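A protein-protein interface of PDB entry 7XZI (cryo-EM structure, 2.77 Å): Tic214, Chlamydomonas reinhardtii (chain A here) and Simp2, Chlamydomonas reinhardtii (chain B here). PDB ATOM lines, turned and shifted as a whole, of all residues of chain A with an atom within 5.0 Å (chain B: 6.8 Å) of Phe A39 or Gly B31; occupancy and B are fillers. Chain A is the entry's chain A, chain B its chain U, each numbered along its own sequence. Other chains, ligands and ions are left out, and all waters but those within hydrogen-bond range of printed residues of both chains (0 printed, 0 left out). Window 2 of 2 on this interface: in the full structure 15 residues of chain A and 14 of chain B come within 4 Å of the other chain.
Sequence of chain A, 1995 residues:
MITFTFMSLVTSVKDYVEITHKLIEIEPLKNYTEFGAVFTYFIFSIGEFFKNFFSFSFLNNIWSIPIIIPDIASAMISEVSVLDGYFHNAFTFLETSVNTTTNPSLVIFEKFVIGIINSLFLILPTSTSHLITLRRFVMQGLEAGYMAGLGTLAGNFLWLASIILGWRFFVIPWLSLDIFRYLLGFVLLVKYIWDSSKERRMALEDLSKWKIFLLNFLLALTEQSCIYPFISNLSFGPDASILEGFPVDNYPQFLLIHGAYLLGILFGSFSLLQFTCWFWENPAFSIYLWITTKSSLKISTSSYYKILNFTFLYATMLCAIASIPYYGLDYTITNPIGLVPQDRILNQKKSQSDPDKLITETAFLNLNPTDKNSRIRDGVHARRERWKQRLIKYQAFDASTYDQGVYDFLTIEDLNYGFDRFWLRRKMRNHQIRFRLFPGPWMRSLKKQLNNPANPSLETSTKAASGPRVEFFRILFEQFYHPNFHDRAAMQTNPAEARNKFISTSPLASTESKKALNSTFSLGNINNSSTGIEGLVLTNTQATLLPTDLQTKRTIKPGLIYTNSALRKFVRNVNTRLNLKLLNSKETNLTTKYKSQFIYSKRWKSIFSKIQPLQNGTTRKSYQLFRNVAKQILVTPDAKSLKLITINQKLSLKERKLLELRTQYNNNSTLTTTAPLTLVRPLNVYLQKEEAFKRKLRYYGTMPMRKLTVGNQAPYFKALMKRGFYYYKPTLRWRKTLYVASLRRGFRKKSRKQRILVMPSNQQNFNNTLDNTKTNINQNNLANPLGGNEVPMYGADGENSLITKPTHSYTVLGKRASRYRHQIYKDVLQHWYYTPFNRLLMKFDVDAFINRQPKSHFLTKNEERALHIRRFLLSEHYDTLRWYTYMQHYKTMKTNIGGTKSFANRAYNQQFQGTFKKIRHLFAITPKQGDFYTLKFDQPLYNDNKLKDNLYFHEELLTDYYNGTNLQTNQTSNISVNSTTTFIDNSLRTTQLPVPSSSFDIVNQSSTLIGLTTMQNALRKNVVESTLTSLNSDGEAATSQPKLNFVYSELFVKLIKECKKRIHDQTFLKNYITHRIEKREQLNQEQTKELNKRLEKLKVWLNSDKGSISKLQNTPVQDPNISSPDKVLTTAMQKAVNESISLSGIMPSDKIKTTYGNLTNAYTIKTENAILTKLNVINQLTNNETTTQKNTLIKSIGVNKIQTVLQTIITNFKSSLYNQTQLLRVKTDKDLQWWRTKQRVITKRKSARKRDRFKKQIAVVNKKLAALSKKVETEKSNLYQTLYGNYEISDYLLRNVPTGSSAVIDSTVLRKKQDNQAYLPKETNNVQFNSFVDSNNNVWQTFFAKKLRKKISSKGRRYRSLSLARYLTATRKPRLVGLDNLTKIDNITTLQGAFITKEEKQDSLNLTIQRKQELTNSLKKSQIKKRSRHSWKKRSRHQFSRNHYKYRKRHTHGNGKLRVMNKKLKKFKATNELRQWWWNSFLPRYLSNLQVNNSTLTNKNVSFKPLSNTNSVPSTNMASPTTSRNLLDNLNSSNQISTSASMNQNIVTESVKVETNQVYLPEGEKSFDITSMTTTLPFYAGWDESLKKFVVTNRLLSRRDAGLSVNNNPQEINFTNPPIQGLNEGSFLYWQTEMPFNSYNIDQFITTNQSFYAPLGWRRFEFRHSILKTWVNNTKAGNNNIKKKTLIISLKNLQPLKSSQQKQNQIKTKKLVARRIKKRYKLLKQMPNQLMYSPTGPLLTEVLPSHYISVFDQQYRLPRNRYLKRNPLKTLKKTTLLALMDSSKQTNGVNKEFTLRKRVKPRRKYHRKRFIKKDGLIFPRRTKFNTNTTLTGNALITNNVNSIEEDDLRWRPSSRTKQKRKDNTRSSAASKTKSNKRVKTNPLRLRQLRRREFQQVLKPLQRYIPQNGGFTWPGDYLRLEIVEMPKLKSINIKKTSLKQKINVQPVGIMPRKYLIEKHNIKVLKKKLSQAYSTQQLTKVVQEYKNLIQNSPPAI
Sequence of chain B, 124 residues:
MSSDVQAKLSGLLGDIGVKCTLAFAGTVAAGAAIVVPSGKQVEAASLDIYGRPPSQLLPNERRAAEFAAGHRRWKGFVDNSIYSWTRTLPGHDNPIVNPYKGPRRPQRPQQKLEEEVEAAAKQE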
ATOM      1  N   GLU A  34     -12.083 -13.782   3.603  1.00  0.00           N
ATOM      2  CA  GLU A  34     -12.362 -15.057   4.244  1.00  0.00           C
ATOM      3  C   GLU A  34     -11.550 -15.176   5.526  1.00  0.00           C
ATOM      4  O   GLU A  34     -10.368 -14.823   5.566  1.00  0.00           O
ATOM      5  CB  GLU A  34     -12.034 -16.219   3.310  1.00  0.00           C
ATOM      6  CG  GLU A  34     -13.112 -16.536   2.298  1.00  0.00           C
ATOM      7  CD  GLU A  34     -12.923 -17.904   1.676  1.00  0.00           C
ATOM      8  OE1 GLU A  34     -12.150 -18.708   2.237  1.00  0.00           O
ATOM      9  OE2 GLU A  34     -13.544 -18.175   0.628  1.00  0.00           O
ATOM     10  N   PHE A  35     -12.192 -15.678   6.581  1.00  0.00           N
ATOM     11  CA  PHE A  35     -11.523 -15.759   7.874  1.00  0.00           C
ATOM     12  C   PHE A  35     -10.332 -16.709   7.830  1.00  0.00           C
ATOM     13  O   PHE A  35      -9.276 -16.412   8.399  1.00  0.00           O
ATOM     14  CB  PHE A  35     -12.515 -16.193   8.952  1.00  0.00           C
ATOM     15  CG  PHE A  35     -11.904 -16.321  10.316  1.00  0.00           C
ATOM     16  CD1 PHE A  35     -11.690 -15.201  11.101  1.00  0.00           C
ATOM     17  CD2 PHE A  35     -11.547 -17.561  10.815  1.00  0.00           C
ATOM     18  CE1 PHE A  35     -11.128 -15.316  12.357  1.00  0.00           C
ATOM     19  CE2 PHE A  35     -10.984 -17.683  12.070  1.00  0.00           C
ATOM     20  CZ  PHE A  35     -10.775 -16.559  12.842  1.00  0.00           C
ATOM     21  N   GLY A  36     -10.482 -17.854   7.163  1.00  0.00           N
ATOM     22  CA  GLY A  36      -9.404 -18.829   7.140  1.00  0.00           C
ATOM     23  C   GLY A  36      -8.160 -18.321   6.437  1.00  0.00           C
ATOM     24  O   GLY A  36      -7.044 -18.465   6.941  1.00  0.00           O
ATOM     25  N   ALA A  37      -8.338 -17.721   5.257  1.00  0.00           N
ATOM     26  CA  ALA A  37      -7.195 -17.232   4.493  1.00  0.00           C
ATOM     27  C   ALA A  37      -6.488 -16.098   5.223  1.00  0.00           C
ATOM     28  O   ALA A  37      -5.255 -16.076   5.313  1.00  0.00           O
ATOM     29  CB  ALA A  37      -7.646 -16.780   3.104  1.00  0.00           C
ATOM     30  N   VAL A  38      -7.257 -15.146   5.754  1.00  0.00           N
ATOM     31  CA  VAL A  38      -6.662 -14.044   6.502  1.00  0.00           C
ATOM     32  C   VAL A  38      -5.923 -14.570   7.724  1.00  0.00           C
ATOM     33  O   VAL A  38      -4.807 -14.132   8.027  1.00  0.00           O
ATOM     34  CB  VAL A  38      -7.742 -13.016   6.888  1.00  0.00           C
ATOM     35  CG1 VAL A  38      -7.166 -11.967   7.823  1.00  0.00           C
ATOM     36  CG2 VAL A  38      -8.315 -12.362   5.644  1.00  0.00           C
ATOM     37  N   PHE A  39      -6.525 -15.525   8.434  1.00  0.00           N
ATOM     38  CA  PHE A  39      -5.902 -16.070   9.635  1.00  0.00           C
ATOM     39  C   PHE A  39      -4.588 -16.769   9.306  1.00  0.00           C
ATOM     40  O   PHE A  39      -3.567 -16.540   9.967  1.00  0.00           O
ATOM     41  CB  PHE A  39      -6.872 -17.031  10.325  1.00  0.00           C
ATOM     42  CG  PHE A  39      -6.369 -17.572  11.633  1.00  0.00           C
ATOM     43  CD1 PHE A  39      -6.488 -16.831  12.797  1.00  0.00           C
ATOM     44  CD2 PHE A  39      -5.791 -18.828  11.702  1.00  0.00           C
ATOM     45  CE1 PHE A  39      -6.031 -17.329  14.002  1.00  0.00           C
ATOM     46  CE2 PHE A  39      -5.333 -19.331  12.903  1.00  0.00           C
ATOM     47  CZ  PHE A  39      -5.453 -18.581  14.055  1.00  0.00           C
ATOM     48  N   THR A  40      -4.591 -17.623   8.280  1.00  0.00           N
ATOM     49  CA  THR A  40      -3.374 -18.358   7.956  1.00  0.00           C
ATOM     50  C   THR A  40      -2.294 -17.429   7.413  1.00  0.00           C
ATOM     51  O   THR A  40      -1.111 -17.606   7.724  1.00  0.00           O
ATOM     52  CB  THR A  40      -3.673 -19.501   6.978  1.00  0.00           C
ATOM     53  OG1 THR A  40      -2.484 -20.274   6.770  1.00  0.00           O
ATOM     54  CG2 THR A  40      -4.168 -18.984   5.642  1.00  0.00           C
ATOM     55  N   TYR A  41      -2.673 -16.416   6.625  1.00  0.00           N
ATOM     56  CA  TYR A  41      -1.673 -15.475   6.132  1.00  0.00           C
ATOM     57  C   TYR A  41      -1.097 -14.639   7.267  1.00  0.00           C
ATOM     58  O   TYR A  41       0.099 -14.333   7.270  1.00  0.00           O
ATOM     59  CB  TYR A  41      -2.268 -14.575   5.051  1.00  0.00           C
ATOM     60  CG  TYR A  41      -1.244 -13.674   4.394  1.00  0.00           C
ATOM     61  CD1 TYR A  41      -0.407 -14.156   3.397  1.00  0.00           C
ATOM     62  CD2 TYR A  41      -1.111 -12.345   4.774  1.00  0.00           C
ATOM     63  CE1 TYR A  41       0.532 -13.339   2.796  1.00  0.00           C
ATOM     64  CE2 TYR A  41      -0.174 -11.521   4.178  1.00  0.00           C
ATOM     65  CZ  TYR A  41       0.643 -12.024   3.189  1.00  0.00           C
ATOM     66  OH  TYR A  41       1.577 -11.210   2.591  1.00  0.00           O
ATOM     67  N   PHE A  42      -1.931 -14.259   8.238  1.00  0.00           N
ATOM     68  CA  PHE A  42      -1.433 -13.534   9.402  1.00  0.00           C
ATOM     69  C   PHE A  42      -0.461 -14.388  10.206  1.00  0.00           C
ATOM     70  O   PHE A  42       0.586 -13.901  10.650  1.00  0.00           O
ATOM     71  CB  PHE A  42      -2.607 -13.081  10.269  1.00  0.00           C
ATOM     72  CG  PHE A  42      -2.208 -12.591  11.631  1.00  0.00           C
ATOM     73  CD1 PHE A  42      -1.696 -11.316  11.802  1.00  0.00           C
ATOM     74  CD2 PHE A  42      -2.360 -13.400  12.744  1.00  0.00           C
ATOM     75  CE1 PHE A  42      -1.333 -10.861  13.056  1.00  0.00           C
ATOM     76  CE2 PHE A  42      -1.999 -12.952  14.000  1.00  0.00           C
ATOM     77  CZ  PHE A  42      -1.485 -11.681  14.156  1.00  0.00           C
ATOM     78  N   ILE A  43      -0.791 -15.667  10.401  1.00  0.00           N
ATOM     79  CA  ILE A  43       0.114 -16.563  11.116  1.00  0.00           C
ATOM     80  C   ILE A  43       1.430 -16.703  10.359  1.00  0.00           C
ATOM     81  O   ILE A  43       2.514 -16.656  10.956  1.00  0.00           O
ATOM     82  CB  ILE A  43      -0.557 -17.930  11.360  1.00  0.00           C
ATOM     83  CG1 ILE A  43      -1.232 -17.964  12.734  1.00  0.00           C
ATOM     84  CG2 ILE A  43       0.456 -19.060  11.261  1.00  0.00           C
ATOM     85  CD1 ILE A  43      -2.384 -17.003  12.893  1.00  0.00           C
ATOM     86  N   GLY B  26      -0.839 -17.529  22.830  1.00  0.00           N
ATOM     87  CA  GLY B  26      -1.327 -18.896  22.748  1.00  0.00           C
ATOM     88  C   GLY B  26      -2.148 -19.150  21.500  1.00  0.00           C
ATOM     89  O   GLY B  26      -2.037 -20.210  20.877  1.00  0.00           O
ATOM     90  N   THR B  27      -2.989 -18.185  21.118  1.00  0.00           N
ATOM     91  CA  THR B  27      -3.748 -18.321  19.879  1.00  0.00           C
ATOM     92  C   THR B  27      -2.819 -18.394  18.674  1.00  0.00           C
ATOM     93  O   THR B  27      -3.019 -19.220  17.774  1.00  0.00           O
ATOM     94  CB  THR B  27      -4.730 -17.158  19.733  1.00  0.00           C
ATOM     95  OG1 THR B  27      -5.637 -17.156  20.842  1.00  0.00           O
ATOM     96  CG2 THR B  27      -5.520 -17.286  18.441  1.00  0.00           C
ATOM     97  N   VAL B  28      -1.789 -17.544  18.647  1.00  0.00           N
ATOM     98  CA  VAL B  28      -0.828 -17.575  17.546  1.00  0.00           C
ATOM     99  C   VAL B  28      -0.093 -18.910  17.512  1.00  0.00           C
ATOM    100  O   VAL B  28       0.126 -19.490  16.442  1.00  0.00           O
ATOM    101  CB  VAL B  28       0.149 -16.390  17.656  1.00  0.00           C
ATOM    102  CG1 VAL B  28       1.271 -16.527  16.639  1.00  0.00           C
ATOM    103  CG2 VAL B  28      -0.589 -15.077  17.454  1.00  0.00           C
ATOM    104  N   ALA B  29       0.306 -19.415  18.682  1.00  0.00           N
ATOM    105  CA  ALA B  29       1.013 -20.690  18.744  1.00  0.00           C
ATOM    106  C   ALA B  29       0.136 -21.835  18.253  1.00  0.00           C
ATOM    107  O   ALA B  29       0.601 -22.703  17.506  1.00  0.00           O
ATOM    108  CB  ALA B  29       1.494 -20.954  20.170  1.00  0.00           C
ATOM    109  N   ALA B  30      -1.135 -21.855  18.661  1.00  0.00           N
ATOM    110  CA  ALA B  30      -2.043 -22.900  18.194  1.00  0.00           C
ATOM    111  C   ALA B  30      -2.258 -22.810  16.689  1.00  0.00           C
ATOM    112  O   ALA B  30      -2.261 -23.834  15.990  1.00  0.00           O
ATOM    113  CB  ALA B  30      -3.375 -22.809  18.936  1.00  0.00           C
ATOM    114  N   GLY B  31      -2.437 -21.593  16.170  1.00  0.00           N
ATOM    115  CA  GLY B  31      -2.591 -21.431  14.734  1.00  0.00           C
ATOM    116  C   GLY B  31      -1.380 -21.925  13.966  1.00  0.00           C
ATOM    117  O   GLY B  31      -1.509 -22.637  12.970  1.00  0.00           O
ATOM    118  N   ALA B  32      -0.182 -21.563  14.431  1.00  0.00           N
ATOM    119  CA  ALA B  32       1.035 -22.031  13.776  1.00  0.00           C
ATOM    120  C   ALA B  32       1.182 -23.541  13.888  1.00  0.00           C
ATOM    121  O   ALA B  32       1.691 -24.186  12.966  1.00  0.00           O
ATOM    122  CB  ALA B  32       2.257 -21.332  14.372  1.00  0.00           C
ATOM    123  N   ALA B  33       0.749 -24.122  15.007  1.00  0.00           N
ATOM    124  CA  ALA B  33       0.814 -25.570  15.156  1.00  0.00           C
ATOM    125  C   ALA B  33      -0.110 -26.268  14.169  1.00  0.00           C
ATOM    126  O   ALA B  33       0.227 -27.333  13.639  1.00  0.00           O
ATOM    127  CB  ALA B  33       0.468 -25.964  16.591  1.00  0.00           C
ATOM    128  N   ILE B  34      -1.282 -25.688  13.906  1.00  0.00           N
ATOM    129  CA  ILE B  34      -2.288 -26.385  13.112  1.00  0.00           C
ATOM    130  C   ILE B  34      -2.294 -26.020  11.626  1.00  0.00           C
ATOM    131  O   ILE B  34      -2.943 -26.724  10.839  1.00  0.00           O
ATOM    132  CB  ILE B  34      -3.698 -26.173  13.703  1.00  0.00           C
ATOM    133  CG1 ILE B  34      -4.107 -24.703  13.609  1.00  0.00           C
ATOM    134  CG2 ILE B  34      -3.749 -26.664  15.142  1.00  0.00           C
ATOM    135  CD1 ILE B  34      -5.558 -24.452  13.945  1.00  0.00           C
ATOM    136  N   VAL B  35      -1.603 -24.955  11.214  1.00  0.00           N
ATOM    137  CA  VAL B  35      -1.640 -24.535   9.813  1.00  0.00           C
ATOM    138  C   VAL B  35      -0.282 -24.564   9.124  1.00  0.00           C
ATOM    139  O   VAL B  35      -0.242 -24.514   7.884  1.00  0.00           O
ATOM    140  CB  VAL B  35      -2.271 -23.136   9.647  1.00  0.00           C
ATOM    141  CG1 VAL B  35      -3.515 -22.992  10.511  1.00  0.00           C
ATOM    142  CG2 VAL B  35      -1.253 -22.041   9.935  1.00  0.00           C
ATOM    143  N   VAL B  36       0.822 -24.636   9.860  1.00  0.00           N
ATOM    144  CA  VAL B  36       2.139 -24.590   9.224  1.00  0.00           C
ATOM    145  C   VAL B  36       2.415 -25.913   8.520  1.00  0.00           C
ATOM    146  O   VAL B  36       2.399 -26.975   9.160  1.00  0.00           O
ATOM    147  CB  VAL B  36       3.247 -24.260  10.237  1.00  0.00           C
ATOM    148  CG1 VAL B  36       4.607 -24.642   9.676  1.00  0.00           C
ATOM    149  CG2 VAL B  36       3.218 -22.780  10.580  1.00  0.00           C
ATOM    150  N   ARG B  73      -4.330 -27.259   4.637  1.00  0.00           N
ATOM    151  CA  ARG B  73      -4.296 -27.861   5.968  1.00  0.00           C
ATOM    152  C   ARG B  73      -5.384 -27.285   6.865  1.00  0.00           C
ATOM    153  O   ARG B  73      -6.029 -28.020   7.622  1.00  0.00           O
ATOM    154  CB  ARG B  73      -2.923 -27.659   6.608  1.00  0.00           C
ATOM    155  CG  ARG B  73      -1.787 -28.374   5.904  1.00  0.00           C
ATOM    156  CD  ARG B  73      -0.954 -29.163   6.896  1.00  0.00           C
ATOM    157  NE  ARG B  73      -0.702 -28.406   8.113  1.00  0.00           N
ATOM    158  CZ  ARG B  73      -0.004 -28.859   9.149  1.00  0.00           C
ATOM    159  NH1 ARG B  73       0.539 -30.065   9.142  1.00  0.00           N
ATOM    160  NH2 ARG B  73       0.154 -28.080  10.214  1.00  0.00           N
ATOM    161  N   TRP B  74      -5.592 -25.969   6.805  1.00  0.00           N
ATOM    162  CA  TRP B  74      -6.611 -25.334   7.635  1.00  0.00           C
ATOM    163  C   TRP B  74      -8.003 -25.836   7.281  1.00  0.00           C
ATOM    164  O   TRP B  74      -8.817 -26.121   8.166  1.00  0.00           O
ATOM    165  CB  TRP B  74      -6.533 -23.814   7.494  1.00  0.00           C
ATOM    166  CG  TRP B  74      -7.777 -23.106   7.942  1.00  0.00           C
ATOM    167  CD1 TRP B  74      -8.794 -22.659   7.150  1.00  0.00           C
ATOM    168  CD2 TRP B  74      -8.139 -22.768   9.287  1.00  0.00           C
ATOM    169  NE1 TRP B  74      -9.765 -22.063   7.918  1.00  0.00           N
ATOM    170  CE2 TRP B  74      -9.386 -22.115   9.233  1.00  0.00           C
ATOM    171  CE3 TRP B  74      -7.528 -22.951  10.531  1.00  0.00           C
ATOM    172  CZ2 TRP B  74     -10.035 -21.647  10.374  1.00  0.00           C
ATOM    173  CZ3 TRP B  74      -8.173 -22.485  11.663  1.00  0.00           C
ATOM    174  CH2 TRP B  74      -9.414 -21.841  11.576  1.00  0.00           C
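Gly A36 touches Trp B74 (CA to NE1, 3.3 Å). Phe A39 touches Gly B31 (CE2 to CA, 3.9 Å). Thr A40 touches Val B35 (OG1 to CG2, 3.8 Å). Ala B32 touches Ile A43 (CA to CG2, 3.9 Å). Ile A43 touches Val B35 (CG2 to CG2, 3.7 Å).
Printed residues of chain B within 4 Å of Gly A36: Trp B74. Val A38 touches none of the printed residues of chain B. Gly B26 touches none of the printed residues of chain A. Gly B31 touches just one residue of chain A: Phe A39. Printed residues of chain A within 4 Å of Ala B32: Ile A43 (3.9 Å). Printed residues of chain A within 4 Å of Trp B74: Gly A36. The nearest residue of chain B that does not touch Phe A39 is Trp B74 (4.4 Å).
Of the 13 printed residues of chain B, 4 touch a printed residue of chain A. Printed residues of chain B that touch a printed residue of chain A: Gly B31, Ala B32, Val B35 and Trp B74. Hydrophobic or aromatic side chains of chain B within 4 Å of the printed part of chain A: Val B35 and Trp B74. Of the 10 printed residues of chain A, 4 touch a printed residue of chain B. Hydrophobic or aromatic side chains of chain A that line the printed part of chain B: Phe A39 and Ile A43. Among the printed residues, 5 pairs touch across the chains.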
